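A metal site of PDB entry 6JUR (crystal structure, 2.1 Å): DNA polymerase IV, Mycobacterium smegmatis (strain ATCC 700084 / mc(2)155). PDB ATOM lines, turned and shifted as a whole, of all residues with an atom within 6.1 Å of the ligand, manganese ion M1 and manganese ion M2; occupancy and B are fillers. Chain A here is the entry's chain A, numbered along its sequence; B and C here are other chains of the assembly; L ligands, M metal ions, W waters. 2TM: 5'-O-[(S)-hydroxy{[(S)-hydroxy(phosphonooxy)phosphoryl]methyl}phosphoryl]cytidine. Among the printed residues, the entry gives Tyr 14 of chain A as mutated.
Manganese ion M1 is bound by the side-chain carboxylate of Asp 107, the side-chain carboxylate of Asp 9, the backbone carbonyl oxygen of Leu 10, an oxygen (O2B) of the ligand and an oxygen (O2G) of the ligand.
Manganese ion M1 has five donor atoms within binding distance.
Lys 159 touches manganese ion M1 (NZ to MN, 3.6 Å).
Of the 22 residues printed, 4 come within 4 Å of manganese ion M1.
O of Leu 10 lies close to NZ of Lys 159, at 3.5 Å.
OE1 of Gln 12 is in hydrogen-bond range of N of Tyr 50, at 2.9 Å.
OP1 of DC 18 of chain C lies within salt-bridge range of the side-chain amino group of Lys 152, 3.3 Å away.
The side-chain amino group (NZ) of Lys 159 is in salt-bridge range of the side-chain carboxylate (OD1) of Asp 11, 2.7 Å away.
NZ of Lys 159 lies within hydrogen-bond range of O of Asp 9, 3.2 Å away.
A ring nitrogen (NE2) of His 7 lies within hydrogen-bond range of the side-chain carboxylate (OE1) of Glu 108 (2.7 Å).
NE of Arg 53 is in hydrogen-bond range of O of Ala 48 (2.9 Å).
The side-chain carboxylate of Glu 108 is in salt-bridge range of the side-chain amino group of Lys 152.
Asp 11 touches the ligand.
Tyr 14 touches the ligand.
N2 of DG 5 of chain B touches O2 of the ligand (3.5 Å).
Hydrophobic or aromatic side chains that line the ligand: Phe 13, Tyr 14 and Tyr 50.
Three residues have an atom within 4 Å of manganese ion M2: Asp 9, Asp 107 and Glu 108.
The side-chain amino group of Lys 152 lies close to an oxygen (O1A) of the ligand, at 3.9 Å.
N of Gln 12 sits close to O2G of the ligand (3.1 Å).
OH of Tyr 50 is in hydrogen-bond range of O1G of the ligand (3.4 Å).
O1G of the ligand lies within salt-bridge range of NH1 of Arg 53 (2.5 Å).
The side-chain amino group (NZ) of Lys 159 sits close to an oxygen (O2G) of the ligand (2.8 Å).
O6 of DG 4 of chain B sits at hydrogen-bond distance from N4 of the ligand (2.6 Å).
A nitrogen (N4) of the ligand is in hydrogen-bond range of N4 of DC 18 of chain C (3.3 Å).
The backbone carbonyl oxygen (O) of Thr 46 is in hydrogen-bond range of an oxygen (O2') of the ligand (2.6 Å).
The backbone NH (N) of Phe 13 sits close to an oxygen (O2B) of the ligand (3.1 Å).
Water W2 lies within hydrogen-bond range of O1G of the ligand (2.5 Å) and NH1 of Arg 53 (3.3 Å).
Water W4 lies within hydrogen-bond range of an oxygen (O3') of the ligand, the backbone NH of Tyr 14, the backbone NH of Phe 13 and the side-chain sulfur of Cys 47.
Water W1 bridges O2 of the ligand (2.8 Å) and OH of Tyr 14 (2.9 Å).
Water W3 bridges O2 of DC 18 of chain C (2.7 Å) and O4' of the ligand (3.3 Å).
Manganese ion M2 is bound by O1A of the ligand (1.8 Å), OD2 of Asp 9 (1.9 Å), OD2 of Asp 107 (2.4 Å), OE2 of Glu 108 (2.4 Å) and OD1 of Asp 107 (2.6 Å).
Manganese ion M2 has five donor atoms within binding distance.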
ATOM      1  N   HIS A   7      25.420   7.811 -23.577  1.00  0.00           N
ATOM      2  CA  HIS A   7      24.814   6.643 -22.973  1.00  0.00           C
ATOM      3  C   HIS A   7      25.407   5.486 -23.818  1.00  0.00           C
ATOM      4  O   HIS A   7      25.156   5.489 -25.056  1.00  0.00           O
ATOM      5  CB  HIS A   7      23.268   6.645 -23.056  1.00  0.00           C
ATOM      6  CG  HIS A   7      22.660   5.398 -22.525  1.00  0.00           C
ATOM      7  ND1 HIS A   7      22.125   4.441 -23.366  1.00  0.00           N
ATOM      8  CD2 HIS A   7      22.543   4.901 -21.234  1.00  0.00           C
ATOM      9  CE1 HIS A   7      21.757   3.385 -22.640  1.00  0.00           C
ATOM     10  NE2 HIS A   7      21.943   3.663 -21.354  1.00  0.00           N
ATOM     11  N   ASP A   9      25.571   1.478 -24.609  1.00  0.00           N
ATOM     12  CA  ASP A   9      24.711   0.360 -24.306  1.00  0.00           C
ATOM     13  C   ASP A   9      25.220  -0.816 -25.201  1.00  0.00           C
ATOM     14  O   ASP A   9      25.184  -0.720 -26.422  1.00  0.00           O
ATOM     15  CB  ASP A   9      23.303   0.762 -24.682  1.00  0.00           C
ATOM     16  CG  ASP A   9      22.257  -0.385 -24.358  1.00  0.00           C
ATOM     17  OD1 ASP A   9      22.552  -1.480 -24.790  1.00  0.00           O
ATOM     18  OD2 ASP A   9      21.240  -0.327 -23.554  1.00  0.00           O
ATOM     19  N   LEU A  10      25.573  -1.948 -24.600  1.00  0.00           N
ATOM     20  CA  LEU A  10      25.982  -3.118 -25.372  1.00  0.00           C
ATOM     21  C   LEU A  10      24.880  -3.783 -26.180  1.00  0.00           C
ATOM     22  O   LEU A  10      23.805  -4.065 -25.598  1.00  0.00           O
ATOM     23  CB  LEU A  10      26.580  -4.174 -24.442  1.00  0.00           C
ATOM     24  CG  LEU A  10      27.905  -3.767 -23.802  1.00  0.00           C
ATOM     25  CD1 LEU A  10      28.153  -4.458 -22.459  1.00  0.00           C
ATOM     26  CD2 LEU A  10      29.019  -4.010 -24.851  1.00  0.00           C
ATOM     27  N   ASP A  11      25.103  -4.046 -27.455  1.00  0.00           N
ATOM     28  CA  ASP A  11      24.003  -4.491 -28.336  1.00  0.00           C
ATOM     29  C   ASP A  11      23.669  -5.976 -28.006  1.00  0.00           C
ATOM     30  O   ASP A  11      24.602  -6.745 -27.754  1.00  0.00           O
ATOM     31  CB  ASP A  11      24.465  -4.402 -29.766  1.00  0.00           C
ATOM     32  CG  ASP A  11      24.658  -2.949 -30.222  1.00  0.00           C
ATOM     33  OD1 ASP A  11      24.144  -1.968 -29.590  1.00  0.00           O
ATOM     34  OD2 ASP A  11      25.256  -2.772 -31.296  1.00  0.00           O
ATOM     35  N   GLN A  12      22.368  -6.347 -27.899  1.00  0.00           N
ATOM     36  CA  GLN A  12      21.916  -7.695 -27.604  1.00  0.00           C
ATOM     37  C   GLN A  12      22.892  -8.405 -26.666  1.00  0.00           C
ATOM     38  O   GLN A  12      23.480  -9.458 -26.996  1.00  0.00           O
ATOM     39  CB  GLN A  12      21.723  -8.528 -28.934  1.00  0.00           C
ATOM     40  CG  GLN A  12      22.933  -8.457 -29.903  1.00  0.00           C
ATOM     41  CD  GLN A  12      22.748  -9.307 -31.107  1.00  0.00           C
ATOM     42  OE1 GLN A  12      21.704  -9.976 -31.273  1.00  0.00           O
ATOM     43  NE2 GLN A  12      23.706  -9.267 -31.988  1.00  0.00           N
ATOM     44  N   PHE A  13      23.044  -7.793 -25.482  1.00  0.00           N
ATOM     45  CA  PHE A  13      24.198  -8.108 -24.666  1.00  0.00           C
ATOM     46  C   PHE A  13      24.405  -9.631 -24.432  1.00  0.00           C
ATOM     47  O   PHE A  13      25.450 -10.122 -24.743  1.00  0.00           O
ATOM     48  CB  PHE A  13      24.095  -7.413 -23.280  1.00  0.00           C
ATOM     49  CG  PHE A  13      25.272  -7.685 -22.357  1.00  0.00           C
ATOM     50  CD1 PHE A  13      26.592  -7.742 -22.902  1.00  0.00           C
ATOM     51  CD2 PHE A  13      25.079  -7.833 -20.995  1.00  0.00           C
ATOM     52  CE1 PHE A  13      27.696  -7.961 -22.076  1.00  0.00           C
ATOM     53  CE2 PHE A  13      26.192  -8.056 -20.172  1.00  0.00           C
ATOM     54  CZ  PHE A  13      27.498  -8.135 -20.702  1.00  0.00           C
ATOM     55  N   TYR A  14      23.433 -10.314 -23.794  1.00  0.00           N
ATOM     56  CA  TYR A  14      23.683 -11.747 -23.480  1.00  0.00           C
ATOM     57  C   TYR A  14      23.912 -12.596 -24.705  1.00  0.00           C
ATOM     58  O   TYR A  14      24.727 -13.503 -24.678  1.00  0.00           O
ATOM     59  CB  TYR A  14      22.555 -12.351 -22.673  1.00  0.00           C
ATOM     60  CG  TYR A  14      22.234 -11.697 -21.312  1.00  0.00           C
ATOM     61  CD1 TYR A  14      23.108 -10.702 -20.697  1.00  0.00           C
ATOM     62  CD2 TYR A  14      21.078 -12.127 -20.607  1.00  0.00           C
ATOM     63  CE1 TYR A  14      22.758 -10.159 -19.475  1.00  0.00           C
ATOM     64  CE2 TYR A  14      20.774 -11.542 -19.430  1.00  0.00           C
ATOM     65  CZ  TYR A  14      21.608 -10.605 -18.891  1.00  0.00           C
ATOM     66  OH  TYR A  14      21.224 -10.131 -17.719  1.00  0.00           O
ATOM     67  N   VAL A  45      12.432 -15.607 -22.081  1.00  0.00           N
ATOM     68  CA  VAL A  45      13.645 -15.229 -22.823  1.00  0.00           C
ATOM     69  C   VAL A  45      14.274 -14.078 -22.085  1.00  0.00           C
ATOM     70  O   VAL A  45      13.604 -13.171 -21.664  1.00  0.00           O
ATOM     71  CB  VAL A  45      13.205 -14.756 -24.236  1.00  0.00           C
ATOM     72  CG1 VAL A  45      14.381 -14.119 -24.979  1.00  0.00           C
ATOM     73  CG2 VAL A  45      12.569 -15.973 -24.982  1.00  0.00           C
ATOM     74  N   THR A  46      15.610 -14.123 -21.938  1.00  0.00           N
ATOM     75  CA  THR A  46      16.409 -13.088 -21.323  1.00  0.00           C
ATOM     76  C   THR A  46      17.238 -12.249 -22.320  1.00  0.00           C
ATOM     77  O   THR A  46      17.549 -11.101 -22.089  1.00  0.00           O
ATOM     78  CB  THR A  46      17.301 -13.918 -20.360  1.00  0.00           C
ATOM     79  OG1 THR A  46      17.632 -13.098 -19.344  1.00  0.00           O
ATOM     80  CG2 THR A  46      18.464 -14.430 -20.939  1.00  0.00           C
ATOM     81  N   CYS A  47      17.435 -12.785 -23.532  1.00  0.00           N
ATOM     82  CA  CYS A  47      17.896 -12.012 -24.652  1.00  0.00           C
ATOM     83  C   CYS A  47      17.634 -12.778 -25.935  1.00  0.00           C
ATOM     84  O   CYS A  47      17.937 -13.955 -26.048  1.00  0.00           O
ATOM     85  CB  CYS A  47      19.467 -11.753 -24.502  1.00  0.00           C
ATOM     86  SG  CYS A  47      20.090 -10.727 -25.787  1.00  0.00           S
ATOM     87  N   ALA A  48      16.999 -12.115 -26.915  1.00  0.00           N
ATOM     88  CA  ALA A  48      16.902 -12.697 -28.253  1.00  0.00           C
ATOM     89  C   ALA A  48      17.900 -12.027 -29.173  1.00  0.00           C
ATOM     90  O   ALA A  48      17.892 -10.839 -29.223  1.00  0.00           O
ATOM     91  CB  ALA A  48      15.464 -12.504 -28.793  1.00  0.00           C
ATOM     92  N   TYR A  50      19.211 -10.518 -32.754  1.00  0.00           N
ATOM     93  CA  TYR A  50      18.410  -9.691 -33.713  1.00  0.00           C
ATOM     94  C   TYR A  50      17.641 -10.567 -34.685  1.00  0.00           C
ATOM     95  O   TYR A  50      16.489 -10.249 -35.049  1.00  0.00           O
ATOM     96  CB  TYR A  50      19.300  -8.725 -34.501  1.00  0.00           C
ATOM     97  CG  TYR A  50      19.956  -7.724 -33.628  1.00  0.00           C
ATOM     98  CD1 TYR A  50      19.234  -7.154 -32.605  1.00  0.00           C
ATOM     99  CD2 TYR A  50      21.307  -7.345 -33.762  1.00  0.00           C
ATOM    100  CE1 TYR A  50      19.774  -6.210 -31.737  1.00  0.00           C
ATOM    101  CE2 TYR A  50      21.879  -6.342 -32.871  1.00  0.00           C
ATOM    102  CZ  TYR A  50      21.097  -5.795 -31.861  1.00  0.00           C
ATOM    103  OH  TYR A  50      21.514  -4.739 -30.893  1.00  0.00           O
ATOM    104  N   ARG A  53      14.529 -11.766 -33.054  1.00  0.00           N
ATOM    105  CA  ARG A  53      13.583 -10.685 -32.914  1.00  0.00           C
ATOM    106  C   ARG A  53      12.803 -10.453 -34.224  1.00  0.00           C
ATOM    107  O   ARG A  53      11.697  -9.944 -34.153  1.00  0.00           O
ATOM    108  CB  ARG A  53      14.346  -9.373 -32.653  1.00  0.00           C
ATOM    109  CG  ARG A  53      15.031  -9.387 -31.309  1.00  0.00           C
ATOM    110  CD  ARG A  53      15.831  -8.076 -31.067  1.00  0.00           C
ATOM    111  NE  ARG A  53      16.681  -8.315 -29.898  1.00  0.00           N
ATOM    112  CZ  ARG A  53      17.312  -7.373 -29.149  1.00  0.00           C
ATOM    113  NH1 ARG A  53      17.176  -6.108 -29.466  1.00  0.00           N
ATOM    114  NH2 ARG A  53      18.096  -7.745 -28.134  1.00  0.00           N
ATOM    115  N   ALA A  59      12.854 -10.171 -25.047  1.00  0.00           N
ATOM    116  CA  ALA A  59      13.103 -10.411 -23.597  1.00  0.00           C
ATOM    117  C   ALA A  59      11.800 -10.233 -22.861  1.00  0.00           C
ATOM    118  O   ALA A  59      11.017  -9.339 -23.181  1.00  0.00           O
ATOM    119  CB  ALA A  59      14.140  -9.450 -23.028  1.00  0.00           C
ATOM    120  N   GLY A  60      11.469 -11.161 -21.988  1.00  0.00           N
ATOM    121  CA  GLY A  60      10.179 -11.061 -21.349  1.00  0.00           C
ATOM    122  C   GLY A  60       9.226 -12.046 -21.911  1.00  0.00           C
ATOM    123  O   GLY A  60       8.345 -12.526 -21.181  1.00  0.00           O
ATOM    124  N   ASP A 107      24.312  -3.965 -18.941  1.00  0.00           N
ATOM    125  CA  ASP A 107      24.704  -3.600 -20.303  1.00  0.00           C
ATOM    126  C   ASP A 107      24.865  -2.120 -20.660  1.00  0.00           C
ATOM    127  O   ASP A 107      25.119  -1.828 -21.828  1.00  0.00           O
ATOM    128  CB  ASP A 107      23.849  -4.267 -21.327  1.00  0.00           C
ATOM    129  CG  ASP A 107      22.534  -3.564 -21.528  1.00  0.00           C
ATOM    130  OD1 ASP A 107      21.935  -3.084 -20.539  1.00  0.00           O
ATOM    131  OD2 ASP A 107      22.023  -3.568 -22.664  1.00  0.00           O
ATOM    132  N   GLU A 108      24.824  -1.211 -19.667  1.00  0.00           N
ATOM    133  CA  GLU A 108      24.777   0.201 -19.961  1.00  0.00           C
ATOM    134  C   GLU A 108      25.518   0.953 -18.966  1.00  0.00           C
ATOM    135  O   GLU A 108      25.513   0.598 -17.795  1.00  0.00           O
ATOM    136  CB  GLU A 108      23.339   0.777 -19.785  1.00  0.00           C
ATOM    137  CG  GLU A 108      22.329   0.107 -20.645  1.00  0.00           C
ATOM    138  CD  GLU A 108      20.880   0.508 -20.315  1.00  0.00           C
ATOM    139  OE1 GLU A 108      20.655   1.699 -20.008  1.00  0.00           O
ATOM    140  OE2 GLU A 108      20.017  -0.384 -20.465  1.00  0.00           O
ATOM    141  N   LYS A 152      19.655   8.412 -23.483  1.00  0.00           N
ATOM    142  CA  LYS A 152      19.143   7.077 -23.509  1.00  0.00           C
ATOM    143  C   LYS A 152      18.139   6.959 -24.655  1.00  0.00           C
ATOM    144  O   LYS A 152      18.107   5.967 -25.336  1.00  0.00           O
ATOM    145  CB  LYS A 152      18.461   6.829 -22.104  1.00  0.00           C
ATOM    146  CG  LYS A 152      17.579   5.579 -22.143  1.00  0.00           C
ATOM    147  CD  LYS A 152      18.423   4.310 -21.995  1.00  0.00           C
ATOM    148  CE  LYS A 152      17.507   3.055 -21.850  1.00  0.00           C
ATOM    149  NZ  LYS A 152      18.330   1.801 -21.803  1.00  0.00           N
ATOM    150  N   LYS A 159      20.999   2.172 -32.117  1.00  0.00           N
ATOM    151  CA  LYS A 159      21.094   0.762 -32.326  1.00  0.00           C
ATOM    152  C   LYS A 159      20.735   0.399 -33.802  1.00  0.00           C
ATOM    153  O   LYS A 159      19.864   1.036 -34.389  1.00  0.00           O
ATOM    154  CB  LYS A 159      20.162  -0.026 -31.443  1.00  0.00           C
ATOM    155  CG  LYS A 159      20.202   0.283 -29.911  1.00  0.00           C
ATOM    156  CD  LYS A 159      21.165  -0.622 -29.258  1.00  0.00           C
ATOM    157  CE  LYS A 159      21.147  -0.667 -27.753  1.00  0.00           C
ATOM    158  NZ  LYS A 159      22.327  -1.619 -27.558  1.00  0.00           N
ATOM    159  P    DG B   4       5.972 -14.785 -15.082  1.00  0.00           P
ATOM    160  OP1  DG B   4       5.436 -15.875 -14.251  1.00  0.00           O
ATOM    161  OP2  DG B   4       5.764 -13.393 -14.668  1.00  0.00           O
ATOM    162  O5'  DG B   4       7.525 -14.975 -15.205  1.00  0.00           O
ATOM    163  C5'  DG B   4       8.089 -16.270 -15.469  1.00  0.00           C
ATOM    164  C4'  DG B   4       9.498 -16.219 -14.928  1.00  0.00           C
ATOM    165  O4'  DG B   4      10.372 -15.373 -15.727  1.00  0.00           O
ATOM    166  C3'  DG B   4       9.541 -15.694 -13.495  1.00  0.00           C
ATOM    167  O3'  DG B   4      10.528 -16.458 -12.833  1.00  0.00           O
ATOM    168  C2'  DG B   4      10.074 -14.275 -13.590  1.00  0.00           C
ATOM    169  C1'  DG B   4      10.794 -14.231 -14.955  1.00  0.00           C
ATOM    170  N9   DG B   4      10.453 -13.052 -15.726  1.00  0.00           N
ATOM    171  C8   DG B   4       9.199 -12.660 -16.136  1.00  0.00           C
ATOM    172  N7   DG B   4       9.197 -11.562 -16.830  1.00  0.00           N
ATOM    173  C5   DG B   4      10.545 -11.213 -16.911  1.00  0.00           C
ATOM    174  C6   DG B   4      11.174 -10.109 -17.538  1.00  0.00           C
ATOM    175  O6   DG B   4      10.657  -9.187 -18.177  1.00  0.00           O
ATOM    176  N1   DG B   4      12.554 -10.086 -17.288  1.00  0.00           N
ATOM    177  C2   DG B   4      13.240 -11.058 -16.604  1.00  0.00           C
ATOM    178  N2   DG B   4      14.560 -10.899 -16.559  1.00  0.00           N
ATOM    179  N3   DG B   4      12.669 -12.119 -16.045  1.00  0.00           N
ATOM    180  C4   DG B   4      11.319 -12.119 -16.211  1.00  0.00           C
ATOM    181  P    DG B   5      10.843 -16.159 -11.257  1.00  0.00           P
ATOM    182  OP1  DG B   5      11.384 -17.436 -10.728  1.00  0.00           O
ATOM    183  OP2  DG B   5       9.644 -15.549 -10.634  1.00  0.00           O
ATOM    184  O5'  DG B   5      12.040 -15.092 -11.309  1.00  0.00           O
ATOM    185  C5'  DG B   5      13.313 -15.451 -11.846  1.00  0.00           C
ATOM    186  C4'  DG B   5      14.243 -14.286 -11.653  1.00  0.00           C
ATOM    187  O4'  DG B   5      13.860 -13.222 -12.564  1.00  0.00           O
ATOM    188  C3'  DG B   5      14.107 -13.684 -10.228  1.00  0.00           C
ATOM    189  O3'  DG B   5      15.453 -13.446  -9.867  1.00  0.00           O
ATOM    190  C2'  DG B   5      13.406 -12.334 -10.443  1.00  0.00           C
ATOM    191  C1'  DG B   5      13.841 -11.989 -11.879  1.00  0.00           C
ATOM    192  N9   DG B   5      12.956 -11.069 -12.585  1.00  0.00           N
ATOM    193  C8   DG B   5      11.573 -11.080 -12.615  1.00  0.00           C
ATOM    194  N7   DG B   5      11.076 -10.089 -13.302  1.00  0.00           N
ATOM    195  C5   DG B   5      12.185  -9.365 -13.742  1.00  0.00           C
ATOM    196  C6   DG B   5      12.274  -8.188 -14.549  1.00  0.00           C
ATOM    197  O6   DG B   5      11.363  -7.523 -15.059  1.00  0.00           O
ATOM    198  N1   DG B   5      13.610  -7.850 -14.802  1.00  0.00           N
ATOM    199  C2   DG B   5      14.708  -8.511 -14.314  1.00  0.00           C
ATOM    200  N2   DG B   5      15.897  -8.003 -14.649  1.00  0.00           N
ATOM    201  N3   DG B   5      14.629  -9.615 -13.586  1.00  0.00           N
ATOM    202  C4   DG B   5      13.357  -9.963 -13.304  1.00  0.00           C
ATOM    203  P    DC C  18      15.899   1.486 -18.660  1.00  0.00           P
ATOM    204  OP1  DC C  18      16.923   2.529 -18.873  1.00  0.00           O
ATOM    205  OP2  DC C  18      14.944   0.988 -19.763  1.00  0.00           O
ATOM    206  O5'  DC C  18      16.609   0.118 -18.163  1.00  0.00           O
ATOM    207  C5'  DC C  18      17.682   0.045 -17.237  1.00  0.00           C
ATOM    208  C4'  DC C  18      18.085  -1.419 -17.180  1.00  0.00           C
ATOM    209  O4'  DC C  18      17.041  -2.215 -16.584  1.00  0.00           O
ATOM    210  C3'  DC C  18      18.418  -2.086 -18.527  1.00  0.00           C
ATOM    211  O3'  DC C  18      19.733  -2.586 -18.385  1.00  0.00           O
ATOM    212  C2'  DC C  18      17.305  -3.097 -18.734  1.00  0.00           C
ATOM    213  C1'  DC C  18      16.927  -3.415 -17.295  1.00  0.00           C
ATOM    214  N1   DC C  18      15.564  -3.884 -17.067  1.00  0.00           N
ATOM    215  C2   DC C  18      15.374  -5.096 -16.371  1.00  0.00           C
ATOM    216  O2   DC C  18      16.358  -5.758 -16.065  1.00  0.00           O
ATOM    217  N3   DC C  18      14.127  -5.554 -16.181  1.00  0.00           N
ATOM    218  C4   DC C  18      13.072  -4.843 -16.608  1.00  0.00           C
ATOM    219  N4   DC C  18      11.851  -5.329 -16.380  1.00  0.00           N
ATOM    220  C5   DC C  18      13.236  -3.580 -17.275  1.00  0.00           C
ATOM    221  C6   DC C  18      14.491  -3.147 -17.477  1.00  0.00           C
HETATM  222  O5' 2TM L   1      18.543  -4.753 -22.413  1.00  0.00           O
HETATM  223  C5' 2TM L   1      18.122  -5.122 -21.184  1.00  0.00           C
HETATM  224  C4' 2TM L   1      18.735  -6.433 -20.731  1.00  0.00           C
HETATM  225  O4' 2TM L   1      18.111  -6.534 -19.445  1.00  0.00           O
HETATM  226  C3' 2TM L   1      18.039  -7.445 -21.580  1.00  0.00           C
HETATM  227  O3' 2TM L   1      18.709  -7.978 -22.687  1.00  0.00           O
HETATM  228  C2' 2TM L   1      17.525  -8.468 -20.641  1.00  0.00           C
HETATM  229  O2' 2TM L   1      18.549  -9.423 -20.407  1.00  0.00           O
HETATM  230  C1' 2TM L   1      17.355  -7.692 -19.339  1.00  0.00           C
HETATM  231  C5  2TM L   1      13.949  -6.349 -19.921  1.00  0.00           C
HETATM  232  C6  2TM L   1      15.296  -6.448 -19.961  1.00  0.00           C
HETATM  233  N1  2TM L   1      15.947  -7.469 -19.317  1.00  0.00           N
HETATM  234  C2  2TM L   1      15.246  -8.377 -18.569  1.00  0.00           C
HETATM  235  N3  2TM L   1      13.956  -8.289 -18.489  1.00  0.00           N
HETATM  236  C4  2TM L   1      13.316  -7.277 -19.184  1.00  0.00           C
HETATM  237  O3G 2TM L   1      18.154  -3.286 -26.680  1.00  0.00           O
HETATM  238  PG  2TM L   1      19.226  -4.206 -27.317  1.00  0.00           P
HETATM  239  O1G 2TM L   1      18.885  -4.430 -28.740  1.00  0.00           O
HETATM  240  O2G 2TM L   1      20.678  -3.847 -27.165  1.00  0.00           O
HETATM  241  O3B 2TM L   1      19.117  -5.554 -26.658  1.00  0.00           O
HETATM  242  PB  2TM L   1      19.055  -5.560 -24.979  1.00  0.00           P
HETATM  243  O1B 2TM L   1      17.952  -6.591 -24.746  1.00  0.00           O
HETATM  244  O2B 2TM L   1      20.671  -5.913 -24.674  1.00  0.00           O
HETATM  245  PA  2TM L   1      18.541  -3.302 -22.901  1.00  0.00           P
HETATM  246  O1A 2TM L   1      18.879  -2.033 -22.062  1.00  0.00           O
HETATM  247  O2A 2TM L   1      16.672  -3.299 -22.878  1.00  0.00           O
HETATM  248  N4  2TM L   1      12.010  -7.125 -19.092  1.00  0.00           N
HETATM  249  O2  2TM L   1      15.839  -9.282 -17.959  1.00  0.00           O
HETATM  250  C1  2TM L   1      18.527  -3.910 -24.504  1.00  0.00           C
HETATM  251 MN    MN M   1      21.651  -3.661 -24.694  1.00  0.00          MN
HETATM  252 MN    MN M   2      20.642  -1.689 -22.336  1.00  0.00          MN
HETATM  253  O   HOH W   1      18.366 -10.155 -17.119  1.00  0.00           O
HETATM  254  O   HOH W   2      17.200  -2.816 -29.691  1.00  0.00           O
HETATM  255  O   HOH W   3      18.879  -6.697 -16.283  1.00  0.00           O
HETATM  256  O   HOH W   4      21.141  -8.862 -23.110  1.00  0.00           O
